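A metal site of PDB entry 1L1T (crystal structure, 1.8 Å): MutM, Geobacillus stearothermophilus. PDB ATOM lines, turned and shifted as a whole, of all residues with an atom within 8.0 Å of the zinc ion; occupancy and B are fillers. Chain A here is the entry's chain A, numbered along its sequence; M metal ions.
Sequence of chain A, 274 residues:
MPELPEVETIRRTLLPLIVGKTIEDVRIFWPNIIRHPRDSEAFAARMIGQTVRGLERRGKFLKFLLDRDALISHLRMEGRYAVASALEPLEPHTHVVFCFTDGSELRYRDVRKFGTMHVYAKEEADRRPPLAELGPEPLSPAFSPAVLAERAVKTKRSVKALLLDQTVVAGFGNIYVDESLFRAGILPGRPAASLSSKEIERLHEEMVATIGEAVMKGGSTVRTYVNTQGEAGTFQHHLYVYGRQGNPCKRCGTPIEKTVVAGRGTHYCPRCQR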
ATOM      1  N   PHE A 182     -14.185   6.771  23.545  1.00  0.00           N
ATOM      2  CA  PHE A 182     -15.465   7.207  24.102  1.00  0.00           C
ATOM      3  C   PHE A 182     -16.301   5.991  24.495  1.00  0.00           C
ATOM      4  O   PHE A 182     -16.869   5.941  25.588  1.00  0.00           O
ATOM      5  CB  PHE A 182     -16.284   8.025  23.085  1.00  0.00           C
ATOM      6  CG  PHE A 182     -17.713   8.246  23.499  1.00  0.00           C
ATOM      7  CD1 PHE A 182     -18.052   9.260  24.397  1.00  0.00           C
ATOM      8  CD2 PHE A 182     -18.730   7.407  23.041  1.00  0.00           C
ATOM      9  CE1 PHE A 182     -19.371   9.431  24.835  1.00  0.00           C
ATOM     10  CE2 PHE A 182     -20.055   7.562  23.465  1.00  0.00           C
ATOM     11  CZ  PHE A 182     -20.372   8.577  24.367  1.00  0.00           C
ATOM     12  N   TYR A 240     -20.069   9.172  17.786  1.00  0.00           N
ATOM     13  CA  TYR A 240     -20.457   9.706  19.088  1.00  0.00           C
ATOM     14  C   TYR A 240     -19.761  11.030  19.426  1.00  0.00           C
ATOM     15  O   TYR A 240     -20.364  11.914  20.048  1.00  0.00           O
ATOM     16  CB  TYR A 240     -20.131   8.698  20.195  1.00  0.00           C
ATOM     17  CG  TYR A 240     -21.053   7.508  20.268  1.00  0.00           C
ATOM     18  CD1 TYR A 240     -22.351   7.645  20.757  1.00  0.00           C
ATOM     19  CD2 TYR A 240     -20.620   6.238  19.874  1.00  0.00           C
ATOM     20  CE1 TYR A 240     -23.207   6.531  20.860  1.00  0.00           C
ATOM     21  CE2 TYR A 240     -21.469   5.120  19.965  1.00  0.00           C
ATOM     22  CZ  TYR A 240     -22.751   5.282  20.455  1.00  0.00           C
ATOM     23  OH  TYR A 240     -23.588   4.187  20.570  1.00  0.00           O
ATOM     24  N   VAL A 241     -18.507  11.181  19.005  1.00  0.00           N
ATOM     25  CA  VAL A 241     -17.758  12.388  19.323  1.00  0.00           C
ATOM     26  C   VAL A 241     -16.988  13.101  18.207  1.00  0.00           C
ATOM     27  O   VAL A 241     -16.929  14.333  18.202  1.00  0.00           O
ATOM     28  CB  VAL A 241     -16.742  12.114  20.478  1.00  0.00           C
ATOM     29  CG1 VAL A 241     -17.490  11.691  21.745  1.00  0.00           C
ATOM     30  CG2 VAL A 241     -15.768  11.016  20.063  1.00  0.00           C
ATOM     31  N   PRO A 248     -24.702  18.084  21.885  1.00  0.00           N
ATOM     32  CA  PRO A 248     -24.934  17.214  23.047  1.00  0.00           C
ATOM     33  C   PRO A 248     -24.538  15.751  22.856  1.00  0.00           C
ATOM     34  O   PRO A 248     -24.715  15.178  21.772  1.00  0.00           O
ATOM     35  CB  PRO A 248     -26.433  17.384  23.316  1.00  0.00           C
ATOM     36  CG  PRO A 248     -26.986  17.669  21.944  1.00  0.00           C
ATOM     37  CD  PRO A 248     -25.964  18.624  21.368  1.00  0.00           C
ATOM     38  N   CYS A 249     -23.984  15.153  23.910  1.00  0.00           N
ATOM     39  CA  CYS A 249     -23.589  13.743  23.881  1.00  0.00           C
ATOM     40  C   CYS A 249     -24.843  12.903  23.651  1.00  0.00           C
ATOM     41  O   CYS A 249     -25.891  13.142  24.246  1.00  0.00           O
ATOM     42  CB  CYS A 249     -22.948  13.351  25.223  1.00  0.00           C
ATOM     43  SG  CYS A 249     -22.501  11.588  25.389  1.00  0.00           S
ATOM     44  N   LYS A 250     -24.733  11.908  22.773  1.00  0.00           N
ATOM     45  CA  LYS A 250     -25.871  11.036  22.470  1.00  0.00           C
ATOM     46  C   LYS A 250     -26.274  10.150  23.646  1.00  0.00           C
ATOM     47  O   LYS A 250     -27.378   9.585  23.642  1.00  0.00           O
ATOM     48  CB  LYS A 250     -25.554  10.158  21.258  1.00  0.00           C
ATOM     49  CG  LYS A 250     -25.313  10.927  19.966  1.00  0.00           C
ATOM     50  CD  LYS A 250     -25.200   9.965  18.783  1.00  0.00           C
ATOM     51  CE  LYS A 250     -24.912  10.689  17.483  1.00  0.00           C
ATOM     52  NZ  LYS A 250     -24.806   9.742  16.333  1.00  0.00           N
ATOM     53  N   ARG A 251     -25.400  10.029  24.634  1.00  0.00           N
ATOM     54  CA  ARG A 251     -25.697   9.184  25.789  1.00  0.00           C
ATOM     55  C   ARG A 251     -26.079   9.927  27.063  1.00  0.00           C
ATOM     56  O   ARG A 251     -26.934   9.443  27.820  1.00  0.00           O
ATOM     57  CB  ARG A 251     -24.517   8.251  26.072  1.00  0.00           C
ATOM     58  CG  ARG A 251     -24.278   7.230  24.976  1.00  0.00           C
ATOM     59  CD  ARG A 251     -23.270   6.152  25.371  1.00  0.00           C
ATOM     60  NE  ARG A 251     -23.711   5.355  26.518  1.00  0.00           N
ATOM     61  CZ  ARG A 251     -23.513   5.701  27.784  1.00  0.00           C
ATOM     62  NH1 ARG A 251     -23.960   4.912  28.760  1.00  0.00           N
ATOM     63  NH2 ARG A 251     -22.868   6.817  28.090  1.00  0.00           N
ATOM     64  N   CYS A 252     -25.481  11.091  27.305  1.00  0.00           N
ATOM     65  CA  CYS A 252     -25.803  11.837  28.527  1.00  0.00           C
ATOM     66  C   CYS A 252     -26.243  13.289  28.306  1.00  0.00           C
ATOM     67  O   CYS A 252     -26.679  13.949  29.240  1.00  0.00           O
ATOM     68  CB  CYS A 252     -24.614  11.828  29.492  1.00  0.00           C
ATOM     69  SG  CYS A 252     -23.232  12.891  29.025  1.00  0.00           S
ATOM     70  N   GLY A 253     -26.113  13.780  27.074  1.00  0.00           N
ATOM     71  CA  GLY A 253     -26.526  15.153  26.793  1.00  0.00           C
ATOM     72  C   GLY A 253     -25.522  16.261  27.103  1.00  0.00           C
ATOM     73  O   GLY A 253     -25.774  17.422  26.780  1.00  0.00           O
ATOM     74  N   THR A 254     -24.402  15.909  27.717  1.00  0.00           N
ATOM     75  CA  THR A 254     -23.353  16.893  28.038  1.00  0.00           C
ATOM     76  C   THR A 254     -22.688  17.338  26.721  1.00  0.00           C
ATOM     77  O   THR A 254     -22.440  16.504  25.841  1.00  0.00           O
ATOM     78  CB  THR A 254     -22.283  16.277  28.969  1.00  0.00           C
ATOM     79  OG1 THR A 254     -22.903  15.814  30.180  1.00  0.00           O
ATOM     80  CG2 THR A 254     -21.204  17.301  29.310  1.00  0.00           C
ATOM     81  N   PRO A 255     -22.371  18.638  26.563  1.00  0.00           N
ATOM     82  CA  PRO A 255     -21.734  19.114  25.331  1.00  0.00           C
ATOM     83  C   PRO A 255     -20.369  18.455  25.080  1.00  0.00           C
ATOM     84  O   PRO A 255     -19.537  18.383  25.981  1.00  0.00           O
ATOM     85  CB  PRO A 255     -21.597  20.619  25.552  1.00  0.00           C
ATOM     86  CG  PRO A 255     -22.732  20.937  26.515  1.00  0.00           C
ATOM     87  CD  PRO A 255     -22.671  19.769  27.469  1.00  0.00           C
ATOM     88  N   ILE A 256     -20.150  17.992  23.849  1.00  0.00           N
ATOM     89  CA  ILE A 256     -18.883  17.355  23.479  1.00  0.00           C
ATOM     90  C   ILE A 256     -17.824  18.449  23.394  1.00  0.00           C
ATOM     91  O   ILE A 256     -18.109  19.567  22.946  1.00  0.00           O
ATOM     92  CB  ILE A 256     -18.998  16.629  22.115  1.00  0.00           C
ATOM     93  CG1 ILE A 256     -20.062  15.531  22.207  1.00  0.00           C
ATOM     94  CG2 ILE A 256     -17.649  16.056  21.693  1.00  0.00           C
ATOM     95  CD1 ILE A 256     -19.829  14.525  23.344  1.00  0.00           C
ATOM     96  N   TYR A 268     -14.138  14.463  22.862  1.00  0.00           N
ATOM     97  CA  TYR A 268     -14.537  13.596  23.982  1.00  0.00           C
ATOM     98  C   TYR A 268     -15.687  14.172  24.817  1.00  0.00           C
ATOM     99  O   TYR A 268     -16.001  15.351  24.702  1.00  0.00           O
ATOM    100  CB  TYR A 268     -13.330  13.395  24.906  1.00  0.00           C
ATOM    101  CG  TYR A 268     -12.886  14.677  25.592  1.00  0.00           C
ATOM    102  CD1 TYR A 268     -13.317  14.982  26.882  1.00  0.00           C
ATOM    103  CD2 TYR A 268     -12.089  15.613  24.913  1.00  0.00           C
ATOM    104  CE1 TYR A 268     -12.968  16.197  27.492  1.00  0.00           C
ATOM    105  CE2 TYR A 268     -11.732  16.826  25.528  1.00  0.00           C
ATOM    106  CZ  TYR A 268     -12.182  17.111  26.805  1.00  0.00           C
ATOM    107  OH  TYR A 268     -11.849  18.300  27.415  1.00  0.00           O
ATOM    108  N   CYS A 269     -16.312  13.314  25.624  1.00  0.00           N
ATOM    109  CA  CYS A 269     -17.394  13.754  26.523  1.00  0.00           C
ATOM    110  C   CYS A 269     -16.778  13.748  27.927  1.00  0.00           C
ATOM    111  O   CYS A 269     -16.318  12.712  28.408  1.00  0.00           O
ATOM    112  CB  CYS A 269     -18.583  12.792  26.508  1.00  0.00           C
ATOM    113  SG  CYS A 269     -19.821  13.208  27.797  1.00  0.00           S
ATOM    114  N   PRO A 270     -16.780  14.908  28.613  1.00  0.00           N
ATOM    115  CA  PRO A 270     -16.206  14.993  29.959  1.00  0.00           C
ATOM    116  C   PRO A 270     -16.944  14.221  31.047  1.00  0.00           C
ATOM    117  O   PRO A 270     -16.418  14.050  32.144  1.00  0.00           O
ATOM    118  CB  PRO A 270     -16.175  16.498  30.211  1.00  0.00           C
ATOM    119  CG  PRO A 270     -17.392  16.974  29.501  1.00  0.00           C
ATOM    120  CD  PRO A 270     -17.331  16.206  28.190  1.00  0.00           C
ATOM    121  N   ARG A 271     -18.168  13.759  30.760  1.00  0.00           N
ATOM    122  CA  ARG A 271     -18.926  12.997  31.754  1.00  0.00           C
ATOM    123  C   ARG A 271     -18.798  11.493  31.555  1.00  0.00           C
ATOM    124  O   ARG A 271     -18.571  10.749  32.515  1.00  0.00           O
ATOM    125  CB  ARG A 271     -20.411  13.391  31.752  1.00  0.00           C
ATOM    126  CG  ARG A 271     -21.245  12.547  32.747  1.00  0.00           C
ATOM    127  CD  ARG A 271     -22.719  12.970  32.845  1.00  0.00           C
ATOM    128  NE  ARG A 271     -23.424  12.132  33.830  1.00  0.00           N
ATOM    129  CZ  ARG A 271     -24.704  12.283  34.186  1.00  0.00           C
ATOM    130  NH1 ARG A 271     -25.227  11.474  35.089  1.00  0.00           N
ATOM    131  NH2 ARG A 271     -25.444  13.242  33.651  1.00  0.00           N
ATOM    132  N   CYS A 272     -18.946  11.031  30.309  1.00  0.00           N
ATOM    133  CA  CYS A 272     -18.861   9.603  30.013  1.00  0.00           C
ATOM    134  C   CYS A 272     -17.438   9.027  30.061  1.00  0.00           C
ATOM    135  O   CYS A 272     -17.265   7.832  30.313  1.00  0.00           O
ATOM    136  CB  CYS A 272     -19.460   9.294  28.629  1.00  0.00           C
ATOM    137  SG  CYS A 272     -21.264   9.475  28.468  1.00  0.00           S
ATOM    138  N   GLN A 273     -16.433   9.867  29.810  1.00  0.00           N
ATOM    139  CA  GLN A 273     -15.049   9.408  29.819  1.00  0.00           C
ATOM    140  C   GLN A 273     -14.301   9.895  31.063  1.00  0.00           C
ATOM    141  O   GLN A 273     -14.403  11.058  31.445  1.00  0.00           O
ATOM    142  CB  GLN A 273     -14.337   9.893  28.550  1.00  0.00           C
ATOM    143  CG  GLN A 273     -14.846   9.210  27.279  1.00  0.00           C
ATOM    144  CD  GLN A 273     -14.378   9.883  25.986  1.00  0.00           C
ATOM    145  OE1 GLN A 273     -15.079  10.718  25.415  1.00  0.00           O
ATOM    146  NE2 GLN A 273     -13.182   9.514  25.537  1.00  0.00           N
HETATM  147 ZN    ZN M   1     -21.685  11.695  27.651  1.00  0.00          ZN
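N of Cys 269 is in hydrogen-bond range of OE1 of Gln 273 (2.9 Å).
The side-chain sulfur (SG) of Cys 269 lies close to the backbone NH (N) of Arg 271 (3.4 Å).
The side-chain sulfur of Cys 249 sits close to the backbone NH of Arg 251, 3.4 Å away.
The side-chain sulfur (SG) of Cys 252 lies close to the side-chain hydroxyl (OG1) of Thr 254 (3.2 Å).
The side-chain sulfur (SG) of Cys 272 sits close to the guanidinium group (NH2) of Arg 251 (3.1 Å).
The backbone NH (N) of Cys 249 is in hydrogen-bond range of the backbone carbonyl oxygen (O) of Thr 254 (2.8 Å).
The zinc ion is bound by the side-chain sulfur (SG) of Cys 252.
The side-chain sulfur (SG) of Cys 272 binds the zinc ion (2.4 Å).
The side-chain sulfur (SG) of Cys 269 binds the zinc ion (2.4 Å).
SG of Cys 249 is bound to the zinc ion.
The zinc ion has four donor atoms within binding distance.
Within 4 Å of the zinc ion: Cys 249, Cys 252, Cys 269 and Cys 272.
The nearest printed residue that does not touch the zinc ion is Phe 182 (4.3 Å).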
